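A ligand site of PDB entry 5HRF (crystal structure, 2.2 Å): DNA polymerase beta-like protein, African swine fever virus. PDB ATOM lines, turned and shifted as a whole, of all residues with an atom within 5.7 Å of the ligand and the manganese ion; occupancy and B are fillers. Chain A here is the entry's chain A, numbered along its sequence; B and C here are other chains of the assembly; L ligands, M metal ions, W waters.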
ATOM      1  N   VAL A  41      28.978 -15.402  25.789  1.00  0.00           N
ATOM      2  CA  VAL A  41      27.513 -15.366  25.831  1.00  0.00           C
ATOM      3  C   VAL A  41      26.991 -16.751  26.196  1.00  0.00           C
ATOM      4  O   VAL A  41      27.744 -17.586  26.709  1.00  0.00           O
ATOM      5  CB  VAL A  41      26.942 -14.829  24.490  1.00  0.00           C
ATOM      6  CG1 VAL A  41      27.378 -13.381  24.267  1.00  0.00           C
ATOM      7  CG2 VAL A  41      27.384 -15.696  23.315  1.00  0.00           C
ATOM      8  N   GLY A  42      25.703 -17.005  25.957  1.00  0.00           N
ATOM      9  CA  GLY A  42      25.116 -18.314  26.201  1.00  0.00           C
ATOM     10  C   GLY A  42      25.066 -18.652  27.678  1.00  0.00           C
ATOM     11  O   GLY A  42      25.058 -17.763  28.535  1.00  0.00           O
ATOM     12  N   SER A  43      25.070 -19.950  27.968  1.00  0.00           N
ATOM     13  CA  SER A  43      24.940 -20.415  29.353  1.00  0.00           C
ATOM     14  C   SER A  43      26.154 -20.045  30.214  1.00  0.00           C
ATOM     15  O   SER A  43      26.023 -19.943  31.423  1.00  0.00           O
ATOM     16  CB  SER A  43      24.693 -21.932  29.402  1.00  0.00           C
ATOM     17  OG  SER A  43      25.583 -22.634  28.568  1.00  0.00           O
ATOM     18  N   LEU A  44      27.313 -19.842  29.596  1.00  0.00           N
ATOM     19  CA  LEU A  44      28.499 -19.380  30.319  1.00  0.00           C
ATOM     20  C   LEU A  44      28.277 -17.996  30.955  1.00  0.00           C
ATOM     21  O   LEU A  44      28.589 -17.790  32.130  1.00  0.00           O
ATOM     22  CB  LEU A  44      29.726 -19.360  29.409  1.00  0.00           C
ATOM     23  CG  LEU A  44      31.100 -19.202  30.082  1.00  0.00           C
ATOM     24  CD1 LEU A  44      32.187 -19.826  29.224  1.00  0.00           C
ATOM     25  CD2 LEU A  44      31.454 -17.744  30.364  1.00  0.00           C
ATOM     26  N   ARG A  46      25.396 -16.753  31.628  1.00  0.00           N
ATOM     27  CA  ARG A  46      24.349 -16.978  32.630  1.00  0.00           C
ATOM     28  C   ARG A  46      24.867 -17.799  33.814  1.00  0.00           C
ATOM     29  O   ARG A  46      24.108 -18.103  34.739  1.00  0.00           O
ATOM     30  CB  ARG A  46      23.141 -17.673  32.006  1.00  0.00           C
ATOM     31  CG  ARG A  46      22.389 -16.837  30.983  1.00  0.00           C
ATOM     32  CD  ARG A  46      20.982 -17.396  30.763  1.00  0.00           C
ATOM     33  NE  ARG A  46      20.988 -18.854  30.613  1.00  0.00           N
ATOM     34  CZ  ARG A  46      21.307 -19.511  29.495  1.00  0.00           C
ATOM     35  NH1 ARG A  46      21.674 -18.871  28.397  1.00  0.00           N
ATOM     36  NH2 ARG A  46      21.258 -20.842  29.487  1.00  0.00           N
ATOM     37  N   MET A  50      26.762 -26.358  34.433  1.00  0.00           N
ATOM     38  CA  MET A  50      27.211 -27.177  33.304  1.00  0.00           C
ATOM     39  C   MET A  50      26.796 -26.524  31.995  1.00  0.00           C
ATOM     40  O   MET A  50      25.753 -25.865  31.917  1.00  0.00           O
ATOM     41  CB  MET A  50      26.631 -28.604  33.369  1.00  0.00           C
ATOM     42  CG  MET A  50      26.966 -29.379  34.632  1.00  0.00           C
ATOM     43  SD  MET A  50      28.713 -29.662  34.986  1.00  0.00           S
ATOM     44  CE  MET A  50      29.331 -30.434  33.506  1.00  0.00           C
ATOM     45  N   LEU A  51      27.617 -26.735  30.972  1.00  0.00           N
ATOM     46  CA  LEU A  51      27.408 -26.127  29.665  1.00  0.00           C
ATOM     47  C   LEU A  51      27.523 -27.193  28.571  1.00  0.00           C
ATOM     48  O   LEU A  51      28.374 -28.090  28.645  1.00  0.00           O
ATOM     49  CB  LEU A  51      28.463 -25.041  29.400  1.00  0.00           C
ATOM     50  CG  LEU A  51      28.942 -24.164  30.555  1.00  0.00           C
ATOM     51  CD1 LEU A  51      30.295 -23.551  30.188  1.00  0.00           C
ATOM     52  CD2 LEU A  51      27.946 -23.072  30.908  1.00  0.00           C
ATOM     53  N   ASN A  52      26.698 -27.088  27.544  1.00  0.00           N
ATOM     54  CA  ASN A  52      26.795 -28.010  26.411  1.00  0.00           C
ATOM     55  C   ASN A  52      27.849 -27.592  25.401  1.00  0.00           C
ATOM     56  O   ASN A  52      28.320 -28.415  24.622  1.00  0.00           O
ATOM     57  CB  ASN A  52      25.418 -28.169  25.760  1.00  0.00           C
ATOM     58  CG  ASN A  52      24.436 -28.846  26.682  1.00  0.00           C
ATOM     59  OD1 ASN A  52      24.713 -29.925  27.207  1.00  0.00           O
ATOM     60  ND2 ASN A  52      23.287 -28.206  26.922  1.00  0.00           N
ATOM     61  N   ASP A  53      28.219 -26.317  25.438  1.00  0.00           N
ATOM     62  CA  ASP A  53      29.202 -25.756  24.514  1.00  0.00           C
ATOM     63  C   ASP A  53      29.638 -24.368  24.978  1.00  0.00           C
ATOM     64  O   ASP A  53      29.041 -23.821  25.917  1.00  0.00           O
ATOM     65  CB  ASP A  53      28.610 -25.658  23.101  1.00  0.00           C
ATOM     66  CG  ASP A  53      27.272 -24.956  23.067  1.00  0.00           C
ATOM     67  OD1 ASP A  53      27.142 -23.882  23.659  1.00  0.00           O
ATOM     68  OD2 ASP A  53      26.343 -25.480  22.424  1.00  0.00           O
ATOM     69  N   VAL A  54      30.646 -23.801  24.319  1.00  0.00           N
ATOM     70  CA  VAL A  54      31.116 -22.440  24.592  1.00  0.00           C
ATOM     71  C   VAL A  54      30.680 -21.491  23.477  1.00  0.00           C
ATOM     72  O   VAL A  54      30.993 -21.712  22.319  1.00  0.00           O
ATOM     73  CB  VAL A  54      32.642 -22.370  24.705  1.00  0.00           C
ATOM     74  CG1 VAL A  54      33.095 -20.928  24.877  1.00  0.00           C
ATOM     75  CG2 VAL A  54      33.132 -23.206  25.871  1.00  0.00           C
ATOM     76  N   ASP A  55      29.944 -20.440  23.839  1.00  0.00           N
ATOM     77  CA  ASP A  55      29.406 -19.466  22.870  1.00  0.00           C
ATOM     78  C   ASP A  55      30.168 -18.146  23.011  1.00  0.00           C
ATOM     79  O   ASP A  55      30.156 -17.539  24.089  1.00  0.00           O
ATOM     80  CB  ASP A  55      27.904 -19.253  23.118  1.00  0.00           C
ATOM     81  CG  ASP A  55      27.072 -20.547  22.983  1.00  0.00           C
ATOM     82  OD1 ASP A  55      27.195 -21.209  21.943  1.00  0.00           O
ATOM     83  OD2 ASP A  55      26.286 -20.902  23.879  1.00  0.00           O
ATOM     84  N   ASP A 104      30.989 -22.178  19.617  1.00  0.00           N
ATOM     85  CA  ASP A 104      30.137 -21.429  18.705  1.00  0.00           C
ATOM     86  C   ASP A 104      30.579 -19.978  18.601  1.00  0.00           C
ATOM     87  O   ASP A 104      30.647 -19.267  19.610  1.00  0.00           O
ATOM     88  CB  ASP A 104      28.688 -21.470  19.165  1.00  0.00           C
ATOM     89  CG  ASP A 104      28.183 -22.888  19.363  1.00  0.00           C
ATOM     90  OD1 ASP A 104      28.565 -23.773  18.559  1.00  0.00           O
ATOM     91  OD2 ASP A 104      27.411 -23.120  20.314  1.00  0.00           O
ATOM     92  N   PHE A 106      29.737 -16.263  16.955  1.00  0.00           N
ATOM     93  CA  PHE A 106      28.728 -15.423  16.345  1.00  0.00           C
ATOM     94  C   PHE A 106      29.335 -14.043  16.095  1.00  0.00           C
ATOM     95  O   PHE A 106      30.266 -13.643  16.798  1.00  0.00           O
ATOM     96  CB  PHE A 106      27.517 -15.304  17.271  1.00  0.00           C
ATOM     97  CG  PHE A 106      26.973 -16.642  17.722  1.00  0.00           C
ATOM     98  CD1 PHE A 106      26.180 -17.397  16.860  1.00  0.00           C
ATOM     99  CD2 PHE A 106      27.251 -17.145  18.986  1.00  0.00           C
ATOM    100  CE1 PHE A 106      25.677 -18.614  17.270  1.00  0.00           C
ATOM    101  CE2 PHE A 106      26.735 -18.367  19.399  1.00  0.00           C
ATOM    102  CZ  PHE A 106      25.958 -19.105  18.526  1.00  0.00           C
ATOM    103  N   HIS A 119      20.205 -11.226  22.837  1.00  0.00           N
ATOM    104  CA  HIS A 119      19.769 -12.428  22.114  1.00  0.00           C
ATOM    105  C   HIS A 119      20.574 -13.669  22.521  1.00  0.00           C
ATOM    106  O   HIS A 119      19.985 -14.670  22.957  1.00  0.00           O
ATOM    107  CB  HIS A 119      19.889 -12.172  20.614  1.00  0.00           C
ATOM    108  CG  HIS A 119      19.780 -13.400  19.764  1.00  0.00           C
ATOM    109  ND1 HIS A 119      18.569 -13.927  19.355  1.00  0.00           N
ATOM    110  CD2 HIS A 119      20.731 -14.187  19.213  1.00  0.00           C
ATOM    111  CE1 HIS A 119      18.795 -14.987  18.610  1.00  0.00           C
ATOM    112  NE2 HIS A 119      20.097 -15.165  18.497  1.00  0.00           N
ATOM    113  N   PHE A 120      21.889 -13.610  22.389  1.00  0.00           N
ATOM    114  CA  PHE A 120      22.746 -14.777  22.641  1.00  0.00           C
ATOM    115  C   PHE A 120      22.949 -15.095  24.124  1.00  0.00           C
ATOM    116  O   PHE A 120      23.523 -16.138  24.442  1.00  0.00           O
ATOM    117  CB  PHE A 120      24.098 -14.626  21.950  1.00  0.00           C
ATOM    118  CG  PHE A 120      24.031 -14.752  20.455  1.00  0.00           C
ATOM    119  CD1 PHE A 120      23.694 -15.969  19.861  1.00  0.00           C
ATOM    120  CD2 PHE A 120      24.309 -13.663  19.627  1.00  0.00           C
ATOM    121  CE1 PHE A 120      23.634 -16.091  18.485  1.00  0.00           C
ATOM    122  CE2 PHE A 120      24.249 -13.785  18.251  1.00  0.00           C
ATOM    123  CZ  PHE A 120      23.906 -15.000  17.670  1.00  0.00           C
ATOM    124  N   THR A 121      22.520 -14.221  25.025  1.00  0.00           N
ATOM    125  CA  THR A 121      22.578 -14.520  26.459  1.00  0.00           C
ATOM    126  C   THR A 121      21.451 -15.499  26.822  1.00  0.00           C
ATOM    127  O   THR A 121      21.639 -16.407  27.632  1.00  0.00           O
ATOM    128  CB  THR A 121      22.494 -13.246  27.336  1.00  0.00           C
ATOM    129  OG1 THR A 121      23.667 -12.455  27.153  1.00  0.00           O
ATOM    130  CG2 THR A 121      22.388 -13.599  28.814  1.00  0.00           C
ATOM    131  N   GLY A 122      20.279 -15.297  26.231  1.00  0.00           N
ATOM    132  CA  GLY A 122      19.132 -16.151  26.518  1.00  0.00           C
ATOM    133  C   GLY A 122      18.687 -16.000  27.966  1.00  0.00           C
ATOM    134  O   GLY A 122      18.886 -14.936  28.554  1.00  0.00           O
ATOM    135  N   PRO A 123      18.075 -17.053  28.544  1.00  0.00           N
ATOM    136  CA  PRO A 123      17.791 -18.339  27.903  1.00  0.00           C
ATOM    137  C   PRO A 123      16.643 -18.223  26.921  1.00  0.00           C
ATOM    138  O   PRO A 123      16.013 -17.167  26.818  1.00  0.00           O
ATOM    139  CB  PRO A 123      17.425 -19.244  29.084  1.00  0.00           C
ATOM    140  CG  PRO A 123      16.894 -18.331  30.114  1.00  0.00           C
ATOM    141  CD  PRO A 123      17.555 -16.989  29.923  1.00  0.00           C
ATOM    142  N   VAL A 124      16.363 -19.304  26.199  1.00  0.00           N
ATOM    143  CA  VAL A 124      15.380 -19.277  25.119  1.00  0.00           C
ATOM    144  C   VAL A 124      13.998 -18.905  25.650  1.00  0.00           C
ATOM    145  O   VAL A 124      13.330 -18.040  25.078  1.00  0.00           O
ATOM    146  CB  VAL A 124      15.304 -20.616  24.356  1.00  0.00           C
ATOM    147  CG1 VAL A 124      14.183 -20.601  23.335  1.00  0.00           C
ATOM    148  CG2 VAL A 124      16.630 -20.890  23.675  1.00  0.00           C
ATOM    149  N   LEU A 127      13.568 -15.161  26.301  1.00  0.00           N
ATOM    150  CA  LEU A 127      13.492 -14.403  25.044  1.00  0.00           C
ATOM    151  C   LEU A 127      12.133 -14.545  24.360  1.00  0.00           C
ATOM    152  O   LEU A 127      11.636 -13.589  23.776  1.00  0.00           O
ATOM    153  CB  LEU A 127      14.603 -14.830  24.076  1.00  0.00           C
ATOM    154  CG  LEU A 127      16.060 -14.568  24.495  1.00  0.00           C
ATOM    155  CD1 LEU A 127      17.011 -15.251  23.530  1.00  0.00           C
ATOM    156  CD2 LEU A 127      16.367 -13.080  24.583  1.00  0.00           C
ATOM    157  N   ARG A 131       9.957 -11.173  23.634  1.00  0.00           N
ATOM    158  CA  ARG A 131       9.615 -10.884  22.248  1.00  0.00           C
ATOM    159  C   ARG A 131       8.112 -10.932  21.973  1.00  0.00           C
ATOM    160  O   ARG A 131       7.596 -10.113  21.200  1.00  0.00           O
ATOM    161  CB  ARG A 131      10.344 -11.852  21.317  1.00  0.00           C
ATOM    162  CG  ARG A 131      11.835 -11.618  21.305  1.00  0.00           C
ATOM    163  CD  ARG A 131      12.565 -12.673  20.499  1.00  0.00           C
ATOM    164  NE  ARG A 131      13.981 -12.344  20.430  1.00  0.00           N
ATOM    165  CZ  ARG A 131      14.820 -12.724  19.470  1.00  0.00           C
ATOM    166  NH1 ARG A 131      14.404 -13.483  18.462  1.00  0.00           N
ATOM    167  NH2 ARG A 131      16.087 -12.339  19.516  1.00  0.00           N
ATOM    168  O5'  DC B   1       6.681 -16.637  19.640  1.00  0.00           O
ATOM    169  C5'  DC B   1       6.948 -15.392  20.317  1.00  0.00           C
ATOM    170  C4'  DC B   1       8.188 -14.737  19.758  1.00  0.00           C
ATOM    171  O4'  DC B   1       9.481 -15.226  20.183  1.00  0.00           O
ATOM    172  C3'  DC B   1       8.296 -14.418  18.269  1.00  0.00           C
ATOM    173  O3'  DC B   1       8.612 -13.033  18.063  1.00  0.00           O
ATOM    174  C2'  DC B   1       9.409 -15.341  17.802  1.00  0.00           C
ATOM    175  C1'  DC B   1      10.280 -15.523  19.043  1.00  0.00           C
ATOM    176  N1   DC B   1      10.812 -16.902  19.207  1.00  0.00           N
ATOM    177  C2   DC B   1      12.189 -17.078  19.365  1.00  0.00           C
ATOM    178  O2   DC B   1      12.916 -16.078  19.377  1.00  0.00           O
ATOM    179  N3   DC B   1      12.681 -18.315  19.497  1.00  0.00           N
ATOM    180  C4   DC B   1      11.856 -19.373  19.465  1.00  0.00           C
ATOM    181  N4   DC B   1      12.395 -20.590  19.600  1.00  0.00           N
ATOM    182  C5   DC B   1      10.449 -19.224  19.296  1.00  0.00           C
ATOM    183  C6   DC B   1       9.977 -17.977  19.172  1.00  0.00           C
ATOM    184  P    DA B   2       8.488 -12.382  16.602  1.00  0.00           P
ATOM    185  OP1  DA B   2       8.404 -10.906  16.770  1.00  0.00           O
ATOM    186  OP2  DA B   2       7.438 -13.100  15.849  1.00  0.00           O
ATOM    187  O5'  DA B   2       9.887 -12.745  15.938  1.00  0.00           O
ATOM    188  C5'  DA B   2      11.109 -12.275  16.544  1.00  0.00           C
ATOM    189  C4'  DA B   2      12.324 -12.866  15.854  1.00  0.00           C
ATOM    190  O4'  DA B   2      12.616 -14.162  16.386  1.00  0.00           O
ATOM    191  C3'  DA B   2      12.223 -13.038  14.334  1.00  0.00           C
ATOM    192  O3'  DA B   2      13.078 -12.069  13.723  1.00  0.00           O
ATOM    193  C2'  DA B   2      12.665 -14.470  14.085  1.00  0.00           C
ATOM    194  C1'  DA B   2      13.310 -14.883  15.398  1.00  0.00           C
ATOM    195  N9   DA B   2      13.187 -16.310  15.709  1.00  0.00           N
ATOM    196  C8   DA B   2      12.059 -17.094  15.664  1.00  0.00           C
ATOM    197  N7   DA B   2      12.277 -18.341  15.972  1.00  0.00           N
ATOM    198  C5   DA B   2      13.637 -18.394  16.227  1.00  0.00           C
ATOM    199  C6   DA B   2      14.492 -19.441  16.613  1.00  0.00           C
ATOM    200  N6   DA B   2      14.077 -20.701  16.811  1.00  0.00           N
ATOM    201  N1   DA B   2      15.801 -19.154  16.780  1.00  0.00           N
ATOM    202  C2   DA B   2      16.211 -17.903  16.581  1.00  0.00           C
ATOM    203  N3   DA B   2      15.512 -16.831  16.221  1.00  0.00           N
ATOM    204  C4   DA B   2      14.215 -17.149  16.063  1.00  0.00           C
ATOM    205  P    DT C   9      24.498 -25.521  15.704  1.00  0.00           P
ATOM    206  OP1  DT C   9      25.482 -25.569  14.596  1.00  0.00           O
ATOM    207  OP2  DT C   9      24.786 -26.280  16.953  1.00  0.00           O
ATOM    208  O5'  DT C   9      24.183 -24.019  16.110  1.00  0.00           O
ATOM    209  C5'  DT C   9      23.732 -23.698  17.437  1.00  0.00           C
ATOM    210  C4'  DT C   9      23.407 -22.233  17.564  1.00  0.00           C
ATOM    211  O4'  DT C   9      22.276 -21.905  16.737  1.00  0.00           O
ATOM    212  C3'  DT C   9      23.027 -21.790  18.971  1.00  0.00           C
ATOM    213  C2'  DT C   9      22.137 -20.592  18.717  1.00  0.00           C
ATOM    214  C1'  DT C   9      21.480 -20.905  17.373  1.00  0.00           C
ATOM    215  N1   DT C   9      20.087 -21.409  17.447  1.00  0.00           N
ATOM    216  C2   DT C   9      19.082 -20.511  17.159  1.00  0.00           C
ATOM    217  O2   DT C   9      19.295 -19.343  16.852  1.00  0.00           O
ATOM    218  N3   DT C   9      17.816 -21.028  17.235  1.00  0.00           N
ATOM    219  C4   DT C   9      17.457 -22.314  17.561  1.00  0.00           C
ATOM    220  O4   DT C   9      16.265 -22.635  17.588  1.00  0.00           O
ATOM    221  C5   DT C   9      18.561 -23.200  17.868  1.00  0.00           C
ATOM    222  C7   DT C   9      18.260 -24.619  18.255  1.00  0.00           C
ATOM    223  C6   DT C   9      19.804 -22.705  17.791  1.00  0.00           C
HETATM  224  P1  LIG L   1      23.822 -24.723  26.416  1.00  0.00           P
HETATM  225  O1  LIG L   1      24.820 -24.379  25.335  1.00  0.00           O
HETATM  226  O2  LIG L   1      22.781 -25.719  25.967  1.00  0.00           O
HETATM  227  O3  LIG L   1      24.510 -25.008  27.712  1.00  0.00           O
HETATM  228  O4  LIG L   1      22.926 -23.430  26.746  1.00  0.00           O
HETATM  229  P2  LIG L   1      22.891 -22.098  25.835  1.00  0.00           P
HETATM  230  O5  LIG L   1      21.910 -21.129  26.439  1.00  0.00           O
HETATM  231  O6  LIG L   1      24.317 -21.747  25.573  1.00  0.00           O
HETATM  232  O7  LIG L   1      22.194 -22.548  24.472  1.00  0.00           O
HETATM  233  P3  LIG L   1      22.830 -22.559  22.999  1.00  0.00           P
HETATM  234  O8  LIG L   1      21.969 -23.588  22.313  1.00  0.00           O
HETATM  235  O9  LIG L   1      24.321 -22.736  23.037  1.00  0.00           O
HETATM  236  O10 LIG L   1      22.436 -21.121  22.432  1.00  0.00           O
HETATM  237  C1  LIG L   1      23.257 -19.984  22.663  1.00  0.00           C
HETATM  238  C2  LIG L   1      22.383 -18.753  22.599  1.00  0.00           C
HETATM  239  O11 LIG L   1      21.717 -18.659  21.348  1.00  0.00           O
HETATM  240  C3  LIG L   1      21.252 -18.771  23.612  1.00  0.00           C
HETATM  241  O12 LIG L   1      21.695 -18.449  24.924  1.00  0.00           O
HETATM  242  C4  LIG L   1      20.305 -17.758  23.004  1.00  0.00           C
HETATM  243  C5  LIG L   1      20.424 -18.081  21.525  1.00  0.00           C
HETATM  244  N1  LIG L   1      19.343 -19.039  21.131  1.00  0.00           N
HETATM  245  C6  LIG L   1      19.419 -20.395  21.133  1.00  0.00           C
HETATM  246  N2  LIG L   1      18.242 -20.952  20.726  1.00  0.00           N
HETATM  247  C7  LIG L   1      17.398 -19.939  20.457  1.00  0.00           C
HETATM  248  C8  LIG L   1      16.017 -19.810  19.992  1.00  0.00           C
HETATM  249  O13 LIG L   1      15.339 -20.817  19.747  1.00  0.00           O
HETATM  250  N3  LIG L   1      15.501 -18.581  19.843  1.00  0.00           N
HETATM  251  C9  LIG L   1      16.221 -17.462  20.109  1.00  0.00           C
HETATM  252  N4  LIG L   1      15.653 -16.247  19.939  1.00  0.00           N
HETATM  253  N5  LIG L   1      17.503 -17.507  20.531  1.00  0.00           N
HETATM  254  C10 LIG L   1      18.134 -18.691  20.725  1.00  0.00           C
HETATM  255 MN    MN M   1      25.716 -22.747  24.510  1.00  0.00          MN
HETATM  256  O   HOH W   1      24.925 -24.042  20.716  1.00  0.00           O
HETATM  257  O   HOH W   2      26.769 -22.510  26.236  1.00  0.00           O
HETATM  258  O   HOH W   3      18.351 -23.399  22.071  1.00  0.00           O
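Of the 24 residues printed, 2 come within 4 Å of the manganese ion.
The nearest printed residue that does not touch the manganese ion is Ser 43 (4.1 Å).
The side-chain carboxylate (OD1) of Asp 55 sits close to the side-chain carboxylate (OD2) of Asp 104 (2.5 Å).
The backbone carbonyl oxygen of Asp 55 is in hydrogen-bond range of the backbone NH of Val 41, 3.0 Å away.
O2 of DC 1 of chain B sits at hydrogen-bond distance from the guanidinium group (NH1) of Arg 131 (3.1 Å).
O of Phe 120 sits at hydrogen-bond distance from N of Gly 42, at 2.8 Å.
The guanidinium group (NH1) of Arg 46 sits at hydrogen-bond distance from the backbone carbonyl oxygen (O) of Thr 121, at 2.6 Å.
The guanidinium group of Arg 131 sits at hydrogen-bond distance from a ring nitrogen (ND1) of His 119 (3.0 Å).
O4' of DA 2 of chain B is in hydrogen-bond range of NH1 of Arg 131 (2.8 Å).
N of Asn 52 lies within hydrogen-bond range of O3 of the ligand (3.0 Å).
The side-chain amide nitrogen of Asn 52 lies within hydrogen-bond range of an oxygen (O2) of the ligand, at 2.7 Å.
O6 of the ligand lies close to N of Ser 43 (3.1 Å).
An oxygen (O3) of the ligand lies within hydrogen-bond range of the side-chain hydroxyl (OG) of Ser 43 (2.7 Å).
O2 of DC 1 of chain B lies within hydrogen-bond range of N4 of the ligand.
O of Phe 120 sits at hydrogen-bond distance from O12 of the ligand, 3.0 Å away.
NH1 of Arg 46 lies within salt-bridge range of O5 of the ligand.
N1 of DA 2 of chain B sits at hydrogen-bond distance from a nitrogen (N3) of the ligand.
An oxygen (O12) of the ligand is in hydrogen-bond range of the backbone carbonyl oxygen of Thr 121 (3.4 Å).
The manganese ion is bound by OD1 of Asp 53 (2.0 Å), O6 of the ligand (2.0 Å), O9 of the ligand (2.0 Å), OD2 of Asp 55 (2.0 Å), water W2 (2.0 Å) and O1 of the ligand (2.0 Å).
The guanidinium group (NH1) of Arg 131 sits close to a nitrogen (N4) of the ligand.
O4 of DT 9 of chain C lies close to an oxygen (O13) of the ligand, at 3.0 Å.
Gly 42 touches the ligand.
Leu 51 touches the ligand.
O of His 119 touches C4 of the ligand, at 3.1 Å.
N of Gly 122 touches O12 of the ligand, at 3.7 Å.
CG2 of Val 124 touches N2 of the ligand, 3.4 Å away.
Leu 127 touches the ligand (CD1 to N5, 3.8 Å).
Within 4 Å of the ligand: Gly 42, Ser 43, Arg 46, Leu 51, Asn 52, Asp 53, Asp 55, His 119, Phe 120, Thr 121, Gly 122, Val 124, Leu 127, Arg 131, DC 1 of chain B, DA 2 of chain B and DT 9 of chain C.
The nearest printed residue that does not touch the ligand is Asp 104 (4.1 Å).
Water W2 lies within hydrogen-bond range of OG of Ser 43 (2.6 Å) and O of Asp 53 (2.6 Å).
Water W1 lies within hydrogen-bond range of OD2 of Asp 53 (2.6 Å), OD2 of Asp 104 (2.7 Å) and O8 of the ligand (3.4 Å).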
